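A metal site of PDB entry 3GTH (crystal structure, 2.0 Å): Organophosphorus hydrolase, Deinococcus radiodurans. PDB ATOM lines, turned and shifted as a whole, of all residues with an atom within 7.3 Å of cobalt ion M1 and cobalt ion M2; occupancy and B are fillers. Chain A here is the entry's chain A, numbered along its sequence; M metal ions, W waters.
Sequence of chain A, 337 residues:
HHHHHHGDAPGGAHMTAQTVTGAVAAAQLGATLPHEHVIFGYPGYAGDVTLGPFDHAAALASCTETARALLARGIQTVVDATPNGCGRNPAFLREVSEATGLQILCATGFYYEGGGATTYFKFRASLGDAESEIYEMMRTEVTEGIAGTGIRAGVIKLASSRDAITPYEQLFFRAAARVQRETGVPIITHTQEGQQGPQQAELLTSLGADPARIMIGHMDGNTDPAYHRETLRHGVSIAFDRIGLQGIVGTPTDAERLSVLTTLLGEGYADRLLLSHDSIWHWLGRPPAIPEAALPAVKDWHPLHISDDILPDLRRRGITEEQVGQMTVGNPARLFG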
ATOM      1  N   HIS A  35       0.101  17.308  14.012  1.00  0.00           N
ATOM      2  CA  HIS A  35       1.531  17.070  13.776  1.00  0.00           C
ATOM      3  C   HIS A  35       2.412  18.158  14.373  1.00  0.00           C
ATOM      4  O   HIS A  35       2.610  19.197  13.769  1.00  0.00           O
ATOM      5  CB  HIS A  35       1.798  16.958  12.266  1.00  0.00           C
ATOM      6  CG  HIS A  35       3.202  16.545  11.935  1.00  0.00           C
ATOM      7  ND1 HIS A  35       3.479  15.533  11.039  1.00  0.00           N
ATOM      8  CD2 HIS A  35       4.400  17.032  12.341  1.00  0.00           C
ATOM      9  CE1 HIS A  35       4.792  15.421  10.915  1.00  0.00           C
ATOM     10  NE2 HIS A  35       5.375  16.319  11.693  1.00  0.00           N
ATOM     11  N   GLU A  36       2.909  17.890  15.566  1.00  0.00           N
ATOM     12  CA  GLU A  36       3.823  18.784  16.290  1.00  0.00           C
ATOM     13  C   GLU A  36       4.902  17.955  17.006  1.00  0.00           C
ATOM     14  O   GLU A  36       4.864  16.722  17.058  1.00  0.00           O
ATOM     15  CB  GLU A  36       3.064  19.581  17.358  1.00  0.00           C
ATOM     16  CG  GLU A  36       1.744  20.254  16.876  1.00  0.00           C
ATOM     17  CD  GLU A  36       1.991  21.378  15.885  1.00  0.00           C
ATOM     18  OE1 GLU A  36       1.104  21.688  15.068  1.00  0.00           O
ATOM     19  OE2 GLU A  36       3.083  21.980  15.933  1.00  0.00           O
ATOM     20  N   HIS A  37       5.882  18.660  17.564  1.00  0.00           N
ATOM     21  CA  HIS A  37       6.955  18.015  18.287  1.00  0.00           C
ATOM     22  C   HIS A  37       7.236  18.784  19.572  1.00  0.00           C
ATOM     23  O   HIS A  37       7.802  19.899  19.514  1.00  0.00           O
ATOM     24  CB  HIS A  37       8.204  18.046  17.423  1.00  0.00           C
ATOM     25  CG  HIS A  37       8.066  17.293  16.156  1.00  0.00           C
ATOM     26  ND1 HIS A  37       8.125  15.903  16.111  1.00  0.00           N
ATOM     27  CD2 HIS A  37       7.874  17.694  14.874  1.00  0.00           C
ATOM     28  CE1 HIS A  37       7.980  15.512  14.870  1.00  0.00           C
ATOM     29  NE2 HIS A  37       7.820  16.572  14.105  1.00  0.00           N
ATOM     30  N   PHE A  40      12.454  17.656  20.062  1.00  0.00           N
ATOM     31  CA  PHE A  40      12.916  17.044  18.851  1.00  0.00           C
ATOM     32  C   PHE A  40      14.398  17.297  18.618  1.00  0.00           C
ATOM     33  O   PHE A  40      14.913  18.364  18.920  1.00  0.00           O
ATOM     34  CB  PHE A  40      12.117  17.583  17.675  1.00  0.00           C
ATOM     35  CG  PHE A  40      12.518  17.003  16.337  1.00  0.00           C
ATOM     36  CD1 PHE A  40      13.643  17.483  15.663  1.00  0.00           C
ATOM     37  CD2 PHE A  40      11.772  15.940  15.766  1.00  0.00           C
ATOM     38  CE1 PHE A  40      14.047  16.957  14.454  1.00  0.00           C
ATOM     39  CE2 PHE A  40      12.176  15.389  14.535  1.00  0.00           C
ATOM     40  CZ  PHE A  40      13.319  15.905  13.875  1.00  0.00           C
ATOM     41  N   ALA A  81       4.513  13.779  16.529  1.00  0.00           N
ATOM     42  CA  ALA A  81       4.958  12.940  15.423  1.00  0.00           C
ATOM     43  C   ALA A  81       6.450  12.584  15.418  1.00  0.00           C
ATOM     44  O   ALA A  81       7.012  12.201  14.390  1.00  0.00           O
ATOM     45  CB  ALA A  81       4.592  13.649  14.103  1.00  0.00           C
ATOM     46  N   THR A  82       7.075  12.726  16.564  1.00  0.00           N
ATOM     47  CA  THR A  82       8.501  12.481  16.651  1.00  0.00           C
ATOM     48  C   THR A  82       8.877  11.022  16.485  1.00  0.00           C
ATOM     49  O   THR A  82       8.446  10.173  17.244  1.00  0.00           O
ATOM     50  CB  THR A  82       9.051  12.972  17.992  1.00  0.00           C
ATOM     51  OG1 THR A  82       8.513  14.269  18.253  1.00  0.00           O
ATOM     52  CG2 THR A  82      10.595  13.055  17.938  1.00  0.00           C
ATOM     53  N   PRO A  83       9.720  10.728  15.500  1.00  0.00           N
ATOM     54  CA  PRO A  83      10.221   9.387  15.164  1.00  0.00           C
ATOM     55  C   PRO A  83      11.057   8.870  16.303  1.00  0.00           C
ATOM     56  O   PRO A  83      11.670   9.647  17.053  1.00  0.00           O
ATOM     57  CB  PRO A  83      11.046   9.616  13.925  1.00  0.00           C
ATOM     58  CG  PRO A  83      10.401  10.755  13.310  1.00  0.00           C
ATOM     59  CD  PRO A  83       9.963  11.668  14.393  1.00  0.00           C
ATOM     60  N   TYR A 111      12.346   7.773  10.860  1.00  0.00           N
ATOM     61  CA  TYR A 111      12.238   8.824   9.871  1.00  0.00           C
ATOM     62  C   TYR A 111      12.678   8.376   8.490  1.00  0.00           C
ATOM     63  O   TYR A 111      13.135   7.268   8.331  1.00  0.00           O
ATOM     64  CB  TYR A 111      13.092  10.052  10.343  1.00  0.00           C
ATOM     65  CG  TYR A 111      12.478  11.396  10.029  1.00  0.00           C
ATOM     66  CD1 TYR A 111      11.130  11.478   9.673  1.00  0.00           C
ATOM     67  CD2 TYR A 111      13.190  12.593  10.191  1.00  0.00           C
ATOM     68  CE1 TYR A 111      10.498  12.681   9.481  1.00  0.00           C
ATOM     69  CE2 TYR A 111      12.537  13.821  10.001  1.00  0.00           C
ATOM     70  CZ  TYR A 111      11.195  13.851   9.647  1.00  0.00           C
ATOM     71  OH  TYR A 111      10.490  15.004   9.475  1.00  0.00           O
ATOM     72  N   TYR A 112      12.532   9.246   7.499  1.00  0.00           N
ATOM     73  CA  TYR A 112      12.920   8.961   6.129  1.00  0.00           C
ATOM     74  C   TYR A 112      14.424   8.714   6.007  1.00  0.00           C
ATOM     75  O   TYR A 112      15.224   9.170   6.834  1.00  0.00           O
ATOM     76  CB  TYR A 112      12.447  10.079   5.180  1.00  0.00           C
ATOM     77  CG  TYR A 112      13.205  11.404   5.202  1.00  0.00           C
ATOM     78  CD1 TYR A 112      14.007  11.795   4.124  1.00  0.00           C
ATOM     79  CD2 TYR A 112      13.117  12.275   6.301  1.00  0.00           C
ATOM     80  CE1 TYR A 112      14.697  12.985   4.127  1.00  0.00           C
ATOM     81  CE2 TYR A 112      13.818  13.489   6.314  1.00  0.00           C
ATOM     82  CZ  TYR A 112      14.607  13.831   5.227  1.00  0.00           C
ATOM     83  OH  TYR A 112      15.343  14.998   5.212  1.00  0.00           O
ATOM     84  N   KCX A 157       4.180   6.597  12.669  1.00  0.00           N
ATOM     85  CA  KCX A 157       4.677   7.662  11.815  1.00  0.00           C
ATOM     86  CB  KCX A 157       5.538   8.651  12.659  1.00  0.00           C
ATOM     87  CG  KCX A 157       6.454   9.638  11.850  1.00  0.00           C
ATOM     88  CD  KCX A 157       5.635  10.689  11.166  1.00  0.00           C
ATOM     89  CE  KCX A 157       6.552  11.726  10.500  1.00  0.00           C
ATOM     90  NZ  KCX A 157       7.119  12.634  11.474  1.00  0.00           N
ATOM     91  C   KCX A 157       5.495   7.013  10.706  1.00  0.00           C
ATOM     92  O   KCX A 157       6.403   6.265  10.956  1.00  0.00           O
ATOM     93  CX  KCX A 157       7.628  13.829  11.168  1.00  0.00           C
ATOM     94  OQ1 KCX A 157       7.599  14.261  10.005  1.00  0.00           O
ATOM     95  OQ2 KCX A 157       8.126  14.565  12.052  1.00  0.00           O
ATOM     96  N   LEU A 158       5.144   7.293   9.479  1.00  0.00           N
ATOM     97  CA  LEU A 158       5.871   6.772   8.346  1.00  0.00           C
ATOM     98  C   LEU A 158       6.447   7.992   7.632  1.00  0.00           C
ATOM     99  O   LEU A 158       5.890   9.094   7.741  1.00  0.00           O
ATOM    100  CB  LEU A 158       4.902   6.051   7.385  1.00  0.00           C
ATOM    101  CG  LEU A 158       4.244   4.756   7.867  1.00  0.00           C
ATOM    102  CD1 LEU A 158       3.279   4.210   6.761  1.00  0.00           C
ATOM    103  CD2 LEU A 158       5.364   3.754   8.181  1.00  0.00           C
ATOM    104  N   ALA A 159       7.520   7.792   6.862  1.00  0.00           N
ATOM    105  CA  ALA A 159       8.148   8.907   6.101  1.00  0.00           C
ATOM    106  C   ALA A 159       8.830   8.400   4.824  1.00  0.00           C
ATOM    107  O   ALA A 159       9.392   7.324   4.793  1.00  0.00           O
ATOM    108  CB  ALA A 159       9.173   9.673   6.968  1.00  0.00           C
ATOM    109  N   THR A 189       1.979  10.554   8.132  1.00  0.00           N
ATOM    110  CA  THR A 189       3.224  10.479   7.426  1.00  0.00           C
ATOM    111  C   THR A 189       3.925  11.789   7.164  1.00  0.00           C
ATOM    112  O   THR A 189       3.359  12.851   7.380  1.00  0.00           O
ATOM    113  CB  THR A 189       3.021   9.845   6.071  1.00  0.00           C
ATOM    114  OG1 THR A 189       2.598  10.850   5.155  1.00  0.00           O
ATOM    115  CG2 THR A 189       1.943   8.777   6.164  1.00  0.00           C
ATOM    116  N   HIS A 190       5.157  11.643   6.669  1.00  0.00           N
ATOM    117  CA  HIS A 190       6.042  12.711   6.247  1.00  0.00           C
ATOM    118  C   HIS A 190       6.278  12.520   4.745  1.00  0.00           C
ATOM    119  O   HIS A 190       6.596  11.415   4.294  1.00  0.00           O
ATOM    120  CB  HIS A 190       7.392  12.598   6.981  1.00  0.00           C
ATOM    121  CG  HIS A 190       8.517  13.369   6.352  1.00  0.00           C
ATOM    122  ND1 HIS A 190       9.151  14.423   6.976  1.00  0.00           N
ATOM    123  CD2 HIS A 190       9.198  13.166   5.194  1.00  0.00           C
ATOM    124  CE1 HIS A 190      10.166  14.832   6.238  1.00  0.00           C
ATOM    125  NE2 HIS A 190      10.219  14.094   5.160  1.00  0.00           N
ATOM    126  N   THR A 191       6.099  13.565   3.978  1.00  0.00           N
ATOM    127  CA  THR A 191       6.438  13.503   2.569  1.00  0.00           C
ATOM    128  C   THR A 191       7.544  14.545   2.506  1.00  0.00           C
ATOM    129  O   THR A 191       7.444  15.586   3.144  1.00  0.00           O
ATOM    130  CB  THR A 191       5.316  13.921   1.602  1.00  0.00           C
ATOM    131  OG1 THR A 191       4.794  15.206   1.977  1.00  0.00           O
ATOM    132  CG2 THR A 191       4.238  12.828   1.574  1.00  0.00           C
ATOM    133  N   GLN A 192       8.587  14.228   1.770  1.00  0.00           N
ATOM    134  CA  GLN A 192       9.759  15.077   1.630  1.00  0.00           C
ATOM    135  C   GLN A 192       9.618  16.003   0.437  1.00  0.00           C
ATOM    136  O   GLN A 192       9.365  15.561  -0.678  1.00  0.00           O
ATOM    137  CB  GLN A 192      10.969  14.190   1.439  1.00  0.00           C
ATOM    138  CG  GLN A 192      12.309  14.890   1.443  1.00  0.00           C
ATOM    139  CD  GLN A 192      12.553  15.689   2.697  1.00  0.00           C
ATOM    140  OE1 GLN A 192      12.010  15.385   3.789  1.00  0.00           O
ATOM    141  NE2 GLN A 192      13.376  16.719   2.566  1.00  0.00           N
ATOM    142  N   GLY A 217       1.049  13.456   5.370  1.00  0.00           N
ATOM    143  CA  GLY A 217       1.574  14.760   5.796  1.00  0.00           C
ATOM    144  C   GLY A 217       2.424  15.570   4.844  1.00  0.00           C
ATOM    145  O   GLY A 217       2.814  15.127   3.755  1.00  0.00           O
ATOM    146  N   HIS A 218       2.736  16.781   5.318  1.00  0.00           N
ATOM    147  CA  HIS A 218       3.517  17.785   4.586  1.00  0.00           C
ATOM    148  C   HIS A 218       3.007  17.963   3.182  1.00  0.00           C
ATOM    149  O   HIS A 218       3.791  18.286   2.270  1.00  0.00           O
ATOM    150  CB  HIS A 218       5.021  17.474   4.582  1.00  0.00           C
ATOM    151  CG  HIS A 218       5.587  17.129   5.921  1.00  0.00           C
ATOM    152  ND1 HIS A 218       4.967  17.477   7.106  1.00  0.00           N
ATOM    153  CD2 HIS A 218       6.660  16.372   6.285  1.00  0.00           C
ATOM    154  CE1 HIS A 218       5.613  16.941   8.123  1.00  0.00           C
ATOM    155  NE2 HIS A 218       6.644  16.263   7.651  1.00  0.00           N
ATOM    156  N   ASP A 241       0.639  20.625   7.235  1.00  0.00           N
ATOM    157  CA  ASP A 241       1.126  20.587   8.590  1.00  0.00           C
ATOM    158  C   ASP A 241       2.444  21.242   8.916  1.00  0.00           C
ATOM    159  O   ASP A 241       3.013  20.953   9.954  1.00  0.00           O
ATOM    160  CB  ASP A 241       1.107  19.148   9.064  1.00  0.00           C
ATOM    161  CG  ASP A 241       1.931  18.230   8.175  1.00  0.00           C
ATOM    162  OD1 ASP A 241       1.722  17.004   8.268  1.00  0.00           O
ATOM    163  OD2 ASP A 241       2.780  18.747   7.388  1.00  0.00           O
ATOM    164  N   ARG A 242       2.915  22.096   8.017  1.00  0.00           N
ATOM    165  CA  ARG A 242       4.137  22.859   8.274  1.00  0.00           C
ATOM    166  C   ARG A 242       3.774  24.364   8.108  1.00  0.00           C
ATOM    167  O   ARG A 242       4.560  25.160   7.591  1.00  0.00           O
ATOM    168  CB  ARG A 242       5.225  22.468   7.278  1.00  0.00           C
ATOM    169  CG  ARG A 242       5.413  20.943   7.166  1.00  0.00           C
ATOM    170  CD  ARG A 242       6.657  20.630   6.369  1.00  0.00           C
ATOM    171  NE  ARG A 242       7.788  20.478   7.271  1.00  0.00           N
ATOM    172  CZ  ARG A 242       9.055  20.600   6.915  1.00  0.00           C
ATOM    173  NH1 ARG A 242       9.364  20.881   5.666  1.00  0.00           N
ATOM    174  NH2 ARG A 242      10.018  20.429   7.814  1.00  0.00           N
ATOM    175  N   HIS A 277       1.490  22.736  12.347  1.00  0.00           N
ATOM    176  CA  HIS A 277       2.701  23.570  12.197  1.00  0.00           C
ATOM    177  C   HIS A 277       4.005  22.784  12.036  1.00  0.00           C
ATOM    178  O   HIS A 277       4.974  23.286  11.450  1.00  0.00           O
ATOM    179  CB  HIS A 277       2.891  24.483  13.441  1.00  0.00           C
ATOM    180  CG  HIS A 277       1.633  25.126  13.959  1.00  0.00           C
ATOM    181  ND1 HIS A 277       1.170  26.337  13.486  1.00  0.00           N
ATOM    182  CD2 HIS A 277       0.737  24.719  14.879  1.00  0.00           C
ATOM    183  CE1 HIS A 277       0.046  26.645  14.093  1.00  0.00           C
ATOM    184  NE2 HIS A 277      -0.244  25.674  14.944  1.00  0.00           N
ATOM    185  N   ASP A 278       4.052  21.598  12.608  1.00  0.00           N
ATOM    186  CA  ASP A 278       5.281  20.755  12.570  1.00  0.00           C
ATOM    187  C   ASP A 278       6.330  21.520  13.413  1.00  0.00           C
ATOM    188  O   ASP A 278       7.523  21.471  13.133  1.00  0.00           O
ATOM    189  CB  ASP A 278       5.805  20.609  11.131  1.00  0.00           C
ATOM    190  CG  ASP A 278       6.860  19.547  11.016  1.00  0.00           C
ATOM    191  OD1 ASP A 278       7.536  19.442   9.968  1.00  0.00           O
ATOM    192  OD2 ASP A 278       7.018  18.807  12.002  1.00  0.00           O
ATOM    193  N   SER A 279       5.862  22.229  14.415  1.00  0.00           N
ATOM    194  CA  SER A 279       6.749  23.044  15.223  1.00  0.00           C
ATOM    195  C   SER A 279       7.539  22.192  16.208  1.00  0.00           C
ATOM    196  O   SER A 279       7.190  21.033  16.467  1.00  0.00           O
ATOM    197  CB  SER A 279       5.904  24.077  16.019  1.00  0.00           C
ATOM    198  OG  SER A 279       5.160  23.490  17.077  1.00  0.00           O
ATOM    199  N   ILE A 280       8.613  22.769  16.745  1.00  0.00           N
ATOM    200  CA  ILE A 280       9.399  22.086  17.755  1.00  0.00           C
ATOM    201  C   ILE A 280       9.412  23.042  18.958  1.00  0.00           C
ATOM    202  O   ILE A 280       9.905  24.165  18.884  1.00  0.00           O
ATOM    203  CB  ILE A 280      10.790  21.758  17.210  1.00  0.00           C
ATOM    204  CG1 ILE A 280      10.663  20.659  16.164  1.00  0.00           C
ATOM    205  CG2 ILE A 280      11.702  21.318  18.336  1.00  0.00           C
ATOM    206  CD1 ILE A 280      11.703  20.737  15.041  1.00  0.00           C
HETATM  207 CO    CO M   1       7.427  16.537  12.019  1.00  0.00          CO
HETATM  208 CO    CO M   2       8.427  15.483   8.727  1.00  0.00          CO
HETATM  209  O   HOH W   1       8.216  16.902  10.491  1.00  0.00           O
HETATM  210  O   HOH W   2       9.616  17.100   7.798  1.00  0.00           O
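Cobalt ion M2 is bound by OQ1 of KCX 157 (2.0 Å), ND1 of His 190 (2.2 Å), water W2 (2.2 Å), NE2 of His 218 (2.2 Å), OH of Tyr 111 (2.2 Å) and water W1 (2.3 Å).
NZ of KCX 157 lies close to O of Ala 81.
A ring nitrogen (ND1) of His 37 is in hydrogen-bond range of the side-chain hydroxyl of Thr 82 (2.7 Å).
N of His 37 is in hydrogen-bond range of O of Ser 279.
A ring nitrogen (NE2) of His 190 lies within hydrogen-bond range of the side-chain amide oxygen (OE1) of Gln 192, 2.6 Å away.
The backbone NH of His 190 lies within hydrogen-bond range of the backbone carbonyl oxygen of Leu 158 (2.9 Å).
OD2 of Asp 241 lies within hydrogen-bond range of ND1 of His 218 (2.5 Å).
The side-chain carboxylate (OD1) of Asp 278 lies within salt-bridge range of the guanidinium group (NE) of Arg 242 (2.9 Å).
The backbone NH (N) of Asp 278 lies within hydrogen-bond range of the backbone carbonyl oxygen (O) of Asp 241, at 2.9 Å.
Cobalt ion M1 is bound by water W1 (1.8 Å), a ring nitrogen (NE2) of His 35 (2.1 Å), OQ2 of KCX 157 (2.1 Å), a ring nitrogen (NE2) of His 37 (2.1 Å) and the side-chain carboxylate of Asp 278 (2.3 Å).
Cobalt ion M1 has five donor atoms within binding distance.
Within 4 Å of cobalt ion M2: Tyr 111, KCX 157, His 190 and His 218.
The nearest printed residue that does not touch cobalt ion M2 is His 35 (4.2 Å).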
